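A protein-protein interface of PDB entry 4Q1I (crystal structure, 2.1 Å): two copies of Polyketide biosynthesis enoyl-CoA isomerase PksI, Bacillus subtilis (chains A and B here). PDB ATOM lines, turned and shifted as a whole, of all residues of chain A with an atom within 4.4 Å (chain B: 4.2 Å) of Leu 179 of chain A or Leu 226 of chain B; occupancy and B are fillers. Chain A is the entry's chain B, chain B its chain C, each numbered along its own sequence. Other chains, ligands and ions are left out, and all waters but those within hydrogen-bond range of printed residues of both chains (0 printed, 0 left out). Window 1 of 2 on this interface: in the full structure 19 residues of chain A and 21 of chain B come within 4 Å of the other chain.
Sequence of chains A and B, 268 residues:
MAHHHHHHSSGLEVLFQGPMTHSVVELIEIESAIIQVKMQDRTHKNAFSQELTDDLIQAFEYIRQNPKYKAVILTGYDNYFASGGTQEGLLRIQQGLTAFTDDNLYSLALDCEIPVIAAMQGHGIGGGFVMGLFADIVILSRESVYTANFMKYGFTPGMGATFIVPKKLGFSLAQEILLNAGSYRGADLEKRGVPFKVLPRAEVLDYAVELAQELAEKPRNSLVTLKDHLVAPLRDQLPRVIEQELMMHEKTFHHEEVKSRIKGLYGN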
ATOM      1  N   MET A 151     -19.779  -5.066   5.284  1.00  0.00           N
ATOM      2  CA  MET A 151     -18.394  -5.540   5.196  1.00  0.00           C
ATOM      3  C   MET A 151     -17.385  -4.589   5.908  1.00  0.00           C
ATOM      4  O   MET A 151     -16.267  -4.999   6.237  1.00  0.00           O
ATOM      5  CB  MET A 151     -17.981  -5.830   3.757  1.00  0.00           C
ATOM      6  CG  MET A 151     -18.808  -7.010   3.118  1.00  0.00           C
ATOM      7  SD  MET A 151     -17.763  -8.477   3.407  1.00  0.00           S
ATOM      8  CE  MET A 151     -16.383  -8.157   2.272  1.00  0.00           C
ATOM      9  N   PRO A 157     -22.604  -9.412   3.867  1.00  0.00           N
ATOM     10  CA  PRO A 157     -23.939  -8.793   3.876  1.00  0.00           C
ATOM     11  C   PRO A 157     -24.983  -9.799   4.263  1.00  0.00           C
ATOM     12  O   PRO A 157     -24.900 -10.961   3.837  1.00  0.00           O
ATOM     13  CB  PRO A 157     -24.128  -8.281   2.416  1.00  0.00           C
ATOM     14  CG  PRO A 157     -22.715  -8.159   1.872  1.00  0.00           C
ATOM     15  CD  PRO A 157     -21.877  -9.205   2.587  1.00  0.00           C
ATOM     16  N   THR A 162     -27.403  -9.688  -0.786  1.00  0.00           N
ATOM     17  CA  THR A 162     -26.702 -10.272  -1.940  1.00  0.00           C
ATOM     18  C   THR A 162     -27.681 -10.681  -3.012  1.00  0.00           C
ATOM     19  O   THR A 162     -27.333 -10.913  -4.194  1.00  0.00           O
ATOM     20  CB  THR A 162     -25.818 -11.456  -1.527  1.00  0.00           C
ATOM     21  OG1 THR A 162     -26.632 -12.565  -1.087  1.00  0.00           O
ATOM     22  CG2 THR A 162     -24.834 -10.999  -0.405  1.00  0.00           C
ATOM     23  N   GLN A 175     -21.829  -5.497  -7.005  1.00  0.00           N
ATOM     24  CA  GLN A 175     -20.510  -6.039  -6.551  1.00  0.00           C
ATOM     25  C   GLN A 175     -19.727  -4.967  -5.787  1.00  0.00           C
ATOM     26  O   GLN A 175     -19.155  -5.205  -4.740  1.00  0.00           O
ATOM     27  CB  GLN A 175     -19.631  -6.507  -7.712  1.00  0.00           C
ATOM     28  CG  GLN A 175     -20.185  -7.807  -8.286  1.00  0.00           C
ATOM     29  CD  GLN A 175     -19.466  -8.243  -9.510  1.00  0.00           C
ATOM     30  OE1 GLN A 175     -19.789  -7.781 -10.627  1.00  0.00           O
ATOM     31  NE2 GLN A 175     -18.476  -9.218  -9.338  1.00  0.00           N
ATOM     32  N   GLU A 176     -19.721  -3.779  -6.337  1.00  0.00           N
ATOM     33  CA  GLU A 176     -19.001  -2.637  -5.737  1.00  0.00           C
ATOM     34  C   GLU A 176     -19.656  -2.271  -4.407  1.00  0.00           C
ATOM     35  O   GLU A 176     -18.984  -2.079  -3.425  1.00  0.00           O
ATOM     36  CB  GLU A 176     -19.128  -1.437  -6.708  1.00  0.00           C
ATOM     37  CG  GLU A 176     -18.499  -0.204  -6.070  1.00  0.00           C
ATOM     38  CD  GLU A 176     -18.585   1.040  -6.906  1.00  0.00           C
ATOM     39  OE1 GLU A 176     -18.288   1.009  -8.109  1.00  0.00           O
ATOM     40  OE2 GLU A 176     -18.983   2.057  -6.322  1.00  0.00           O
ATOM     41  N   ILE A 177     -20.989  -2.126  -4.389  1.00  0.00           N
ATOM     42  CA  ILE A 177     -21.735  -1.767  -3.178  1.00  0.00           C
ATOM     43  C   ILE A 177     -21.487  -2.773  -2.016  1.00  0.00           C
ATOM     44  O   ILE A 177     -21.248  -2.349  -0.866  1.00  0.00           O
ATOM     45  CB  ILE A 177     -23.290  -1.625  -3.500  1.00  0.00           C
ATOM     46  CG1 ILE A 177     -23.550  -0.358  -4.385  1.00  0.00           C
ATOM     47  CG2 ILE A 177     -24.143  -1.631  -2.234  1.00  0.00           C
ATOM     48  CD1 ILE A 177     -24.973  -0.128  -4.896  1.00  0.00           C
ATOM     49  N   LEU A 178     -21.569  -4.075  -2.325  1.00  0.00           N
ATOM     50  CA  LEU A 178     -21.545  -5.197  -1.390  1.00  0.00           C
ATOM     51  C   LEU A 178     -20.083  -5.490  -0.942  1.00  0.00           C
ATOM     52  O   LEU A 178     -19.832  -5.553   0.290  1.00  0.00           O
ATOM     53  CB  LEU A 178     -22.114  -6.488  -2.029  1.00  0.00           C
ATOM     54  CG  LEU A 178     -23.625  -6.319  -2.216  1.00  0.00           C
ATOM     55  CD1 LEU A 178     -24.183  -7.438  -3.118  1.00  0.00           C
ATOM     56  CD2 LEU A 178     -24.366  -6.151  -0.880  1.00  0.00           C
ATOM     57  N   LEU A 179     -19.133  -5.567  -1.895  1.00  0.00           N
ATOM     58  CA  LEU A 179     -17.721  -5.876  -1.543  1.00  0.00           C
ATOM     59  C   LEU A 179     -17.068  -4.751  -0.728  1.00  0.00           C
ATOM     60  O   LEU A 179     -16.389  -5.041   0.223  1.00  0.00           O
ATOM     61  CB  LEU A 179     -16.822  -6.126  -2.739  1.00  0.00           C
ATOM     62  CG  LEU A 179     -16.949  -7.464  -3.483  1.00  0.00           C
ATOM     63  CD1 LEU A 179     -16.300  -7.312  -4.855  1.00  0.00           C
ATOM     64  CD2 LEU A 179     -16.365  -8.612  -2.665  1.00  0.00           C
ATOM     65  N   ASN A 180     -17.352  -3.493  -1.066  1.00  0.00           N
ATOM     66  CA  ASN A 180     -16.596  -2.394  -0.512  1.00  0.00           C
ATOM     67  C   ASN A 180     -17.288  -1.624   0.578  1.00  0.00           C
ATOM     68  O   ASN A 180     -16.628  -0.956   1.395  1.00  0.00           O
ATOM     69  CB  ASN A 180     -16.118  -1.458  -1.593  1.00  0.00           C
ATOM     70  CG  ASN A 180     -15.133  -0.464  -1.068  1.00  0.00           C
ATOM     71  OD1 ASN A 180     -14.138  -0.839  -0.357  1.00  0.00           O
ATOM     72  ND2 ASN A 180     -15.389   0.821  -1.371  1.00  0.00           N
ATOM     73  N   ALA A 181     -18.595  -1.795   0.663  1.00  0.00           N
ATOM     74  CA  ALA A 181     -19.349  -1.264   1.760  1.00  0.00           C
ATOM     75  C   ALA A 181     -19.225   0.262   1.819  1.00  0.00           C
ATOM     76  O   ALA A 181     -19.311   0.833   2.901  1.00  0.00           O
ATOM     77  CB  ALA A 181     -18.897  -1.901   3.127  1.00  0.00           C
ATOM     78  N   MET A 248     -22.510 -17.722   5.075  1.00  0.00           N
ATOM     79  CA  MET A 248     -21.361 -16.789   5.067  1.00  0.00           C
ATOM     80  C   MET A 248     -21.165 -16.154   6.435  1.00  0.00           C
ATOM     81  O   MET A 248     -19.996 -15.993   6.869  1.00  0.00           O
ATOM     82  CB  MET A 248     -21.503 -15.695   3.976  1.00  0.00           C
ATOM     83  CG  MET A 248     -21.516 -16.335   2.597  1.00  0.00           C
ATOM     84  SD  MET A 248     -21.306 -15.051   1.306  1.00  0.00           S
ATOM     85  CE  MET A 248     -22.944 -14.265   1.287  1.00  0.00           C
ATOM     86  N   LEU B 215     -10.891  -1.374  -0.373  1.00  0.00           N
ATOM     87  CA  LEU B 215     -11.190  -2.816  -0.338  1.00  0.00           C
ATOM     88  C   LEU B 215     -10.279  -3.538   0.666  1.00  0.00           C
ATOM     89  O   LEU B 215     -10.732  -4.462   1.410  1.00  0.00           O
ATOM     90  CB  LEU B 215     -11.077  -3.464  -1.745  1.00  0.00           C
ATOM     91  CG  LEU B 215     -12.192  -3.167  -2.768  1.00  0.00           C
ATOM     92  CD1 LEU B 215     -11.767  -3.581  -4.183  1.00  0.00           C
ATOM     93  CD2 LEU B 215     -13.467  -3.922  -2.348  1.00  0.00           C
ATOM     94  N   LYS B 218     -10.883  -4.460   4.459  1.00  0.00           N
ATOM     95  CA  LYS B 218     -11.688  -5.613   4.891  1.00  0.00           C
ATOM     96  C   LYS B 218     -10.744  -6.790   5.184  1.00  0.00           C
ATOM     97  O   LYS B 218      -9.734  -6.895   4.552  1.00  0.00           O
ATOM     98  CB  LYS B 218     -12.718  -6.120   3.812  1.00  0.00           C
ATOM     99  CG  LYS B 218     -14.008  -5.291   3.648  1.00  0.00           C
ATOM    100  CD  LYS B 218     -13.640  -3.837   3.395  1.00  0.00           C
ATOM    101  CE  LYS B 218     -14.768  -2.920   2.937  1.00  0.00           C
ATOM    102  NZ  LYS B 218     -14.135  -1.611   2.513  1.00  0.00           N
ATOM    103  N   SER B 222     -13.345 -12.364   4.575  1.00  0.00           N
ATOM    104  CA  SER B 222     -14.612 -11.741   4.215  1.00  0.00           C
ATOM    105  C   SER B 222     -14.762 -11.445   2.749  1.00  0.00           C
ATOM    106  O   SER B 222     -15.822 -11.763   2.101  1.00  0.00           O
ATOM    107  CB  SER B 222     -14.847 -10.487   5.008  1.00  0.00           C
ATOM    108  OG  SER B 222     -15.167 -10.967   6.290  1.00  0.00           O
ATOM    109  N   LEU B 223     -13.698 -10.895   2.207  1.00  0.00           N
ATOM    110  CA  LEU B 223     -13.667 -10.562   0.807  1.00  0.00           C
ATOM    111  C   LEU B 223     -13.871 -11.788  -0.140  1.00  0.00           C
ATOM    112  O   LEU B 223     -14.637 -11.705  -1.099  1.00  0.00           O
ATOM    113  CB  LEU B 223     -12.318  -9.850   0.519  1.00  0.00           C
ATOM    114  CG  LEU B 223     -12.260  -8.385   1.019  1.00  0.00           C
ATOM    115  CD1 LEU B 223     -10.852  -7.956   0.739  1.00  0.00           C
ATOM    116  CD2 LEU B 223     -13.246  -7.408   0.240  1.00  0.00           C
ATOM    117  N   VAL B 224     -13.088 -12.842   0.084  1.00  0.00           N
ATOM    118  CA  VAL B 224     -13.065 -14.127  -0.655  1.00  0.00           C
ATOM    119  C   VAL B 224     -14.387 -14.867  -0.453  1.00  0.00           C
ATOM    120  O   VAL B 224     -14.990 -15.379  -1.437  1.00  0.00           O
ATOM    121  CB  VAL B 224     -11.874 -15.079  -0.129  1.00  0.00           C
ATOM    122  CG1 VAL B 224     -11.821 -16.437  -0.914  1.00  0.00           C
ATOM    123  CG2 VAL B 224     -10.560 -14.350  -0.305  1.00  0.00           C
ATOM    124  N   THR B 225     -14.875 -14.897   0.787  1.00  0.00           N
ATOM    125  CA  THR B 225     -16.216 -15.558   1.059  1.00  0.00           C
ATOM    126  C   THR B 225     -17.281 -14.845   0.220  1.00  0.00           C
ATOM    127  O   THR B 225     -18.094 -15.505  -0.476  1.00  0.00           O
ATOM    128  CB  THR B 225     -16.572 -15.513   2.546  1.00  0.00           C
ATOM    129  OG1 THR B 225     -15.546 -16.184   3.227  1.00  0.00           O
ATOM    130  CG2 THR B 225     -17.870 -16.217   2.931  1.00  0.00           C
ATOM    131  N   LEU B 226     -17.273 -13.515   0.219  1.00  0.00           N
ATOM    132  CA  LEU B 226     -18.337 -12.793  -0.531  1.00  0.00           C
ATOM    133  C   LEU B 226     -18.237 -12.956  -2.080  1.00  0.00           C
ATOM    134  O   LEU B 226     -19.259 -13.150  -2.812  1.00  0.00           O
ATOM    135  CB  LEU B 226     -18.378 -11.284  -0.136  1.00  0.00           C
ATOM    136  CG  LEU B 226     -19.550 -10.542  -0.853  1.00  0.00           C
ATOM    137  CD1 LEU B 226     -20.952 -11.218  -0.649  1.00  0.00           C
ATOM    138  CD2 LEU B 226     -19.517  -9.060  -0.367  1.00  0.00           C
ATOM    139  N   LYS B 227     -17.007 -12.883  -2.566  1.00  0.00           N
ATOM    140  CA  LYS B 227     -16.723 -12.978  -3.963  1.00  0.00           C
ATOM    141  C   LYS B 227     -17.125 -14.378  -4.388  1.00  0.00           C
ATOM    142  O   LYS B 227     -17.832 -14.504  -5.409  1.00  0.00           O
ATOM    143  CB  LYS B 227     -15.228 -12.680  -4.295  1.00  0.00           C
ATOM    144  CG  LYS B 227     -14.943 -12.973  -5.788  1.00  0.00           C
ATOM    145  CD  LYS B 227     -13.539 -12.565  -6.271  1.00  0.00           C
ATOM    146  CE  LYS B 227     -13.429 -12.952  -7.771  1.00  0.00           C
ATOM    147  NZ  LYS B 227     -12.189 -12.422  -8.356  1.00  0.00           N
ATOM    148  N   ASP B 228     -16.782 -15.401  -3.577  1.00  0.00           N
ATOM    149  CA  ASP B 228     -17.105 -16.815  -3.926  1.00  0.00           C
ATOM    150  C   ASP B 228     -18.612 -16.868  -4.157  1.00  0.00           C
ATOM    151  O   ASP B 228     -19.096 -17.473  -5.141  1.00  0.00           O
ATOM    152  CB  ASP B 228     -16.762 -17.801  -2.775  1.00  0.00           C
ATOM    153  CG  ASP B 228     -15.258 -18.218  -2.743  1.00  0.00           C
ATOM    154  OD1 ASP B 228     -14.454 -17.964  -3.694  1.00  0.00           O
ATOM    155  OD2 ASP B 228     -14.890 -18.746  -1.709  1.00  0.00           O
ATOM    156  N   HIS B 229     -19.350 -16.210  -3.247  1.00  0.00           N
ATOM    157  CA  HIS B 229     -20.838 -16.206  -3.334  1.00  0.00           C
ATOM    158  C   HIS B 229     -21.380 -15.472  -4.598  1.00  0.00           C
ATOM    159  O   HIS B 229     -22.221 -15.989  -5.337  1.00  0.00           O
ATOM    160  CB  HIS B 229     -21.423 -15.642  -1.985  1.00  0.00           C
ATOM    161  CG  HIS B 229     -22.899 -15.374  -1.989  1.00  0.00           C
ATOM    162  ND1 HIS B 229     -23.843 -16.378  -1.941  1.00  0.00           N
ATOM    163  CD2 HIS B 229     -23.604 -14.211  -2.052  1.00  0.00           C
ATOM    164  CE1 HIS B 229     -25.060 -15.862  -1.936  1.00  0.00           C
ATOM    165  NE2 HIS B 229     -24.946 -14.543  -1.983  1.00  0.00           N
ATOM    166  N   LEU B 230     -20.930 -14.244  -4.811  1.00  0.00           N
ATOM    167  CA  LEU B 230     -21.329 -13.418  -5.957  1.00  0.00           C
ATOM    168  C   LEU B 230     -20.990 -13.986  -7.336  1.00  0.00           C
ATOM    169  O   LEU B 230     -21.797 -13.853  -8.235  1.00  0.00           O
ATOM    170  CB  LEU B 230     -20.844 -11.939  -5.844  1.00  0.00           C
ATOM    171  CG  LEU B 230     -21.307 -11.204  -4.555  1.00  0.00           C
ATOM    172  CD1 LEU B 230     -20.555  -9.889  -4.322  1.00  0.00           C
ATOM    173  CD2 LEU B 230     -22.808 -10.961  -4.712  1.00  0.00           C
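The side-chain amino group (NZ) of Lys 218 of chain B lies within hydrogen-bond range of the backbone carbonyl oxygen (O) of Asn 180 of chain A, at 2.8 Å. OD1 of Asn 180 of chain A is in hydrogen-bond range of N of Leu 215 of chain B, 3.3 Å away. The side-chain sulfur (SD) of Met 248 of chain A lies close to the backbone carbonyl oxygen (O) of Thr 225 of chain B (3.7 Å). The side-chain hydroxyl of Thr 162 of chain A lies within hydrogen-bond range of a ring nitrogen (NE2) of His 229 of chain B.
Among the printed residues, pairs that only touch across the chains: Met 248 of chain A with His 229 of chain B, Met 151 of chain A with Lys 218 of chain B, Leu 178 of chain A with Leu 226 of chain B, Met 151 of chain A with Ser 222 of chain B, Pro 157 of chain A with Leu 226 of chain B, Leu 179 of chain A with Lys 218 of chain B, Met 151 of chain A with Leu 223 of chain B, Leu 179 of chain A with Leu 226 of chain B, Leu 179 of chain A with Leu 223 of chain B and Thr 162 of chain A with Leu 226 of chain B.
Of chain A, only Pro 157 (3.8 Å), Thr 162 (3.9 Å), Leu 178 (3.6 Å) and Leu 179 (3.8 Å) come within 4 Å of Leu 226 of chain B. Printed residues of chain B within 4 Å of Asn 180 of chain A: Leu 215 (3.3 Å) and Lys 218 (2.8 Å). Of the printed residues of chain B, Pro 157 of chain A touches Leu 226 (3.8 Å). Printed residues of chain B within 4 Å of Met 151 of chain A: Lys 218, Ser 222 and Leu 223. Printed residues of chain A within 4 Å of Thr 225 of chain B: Met 248. Of the printed residues of chain B, Thr 162 of chain A touches Leu 226 (3.9 Å) and His 229 (2.7 Å). Leu 230 of chain B touches none of the printed residues of chain A. The nearest printed residue of chain B that does not touch Thr 162 of chain A is Leu 230 of chain B (4.4 Å).
Hydrophobic or aromatic side chains of chain A that line the printed part of chain B: Met 151, Pro 157, Leu 179 and Met 248. Of the 11 printed residues of chain B, 7 touch a printed residue of chain A. Among the printed residues, no Asp or Glu carboxylate lies within 4 Å of a Lys or Arg side-chain nitrogen of the other chain.
No position is printed for both chains. Of the 14 pairs that touch across the chains among the printed residues, none has its exchanged pair printed and touching as well.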
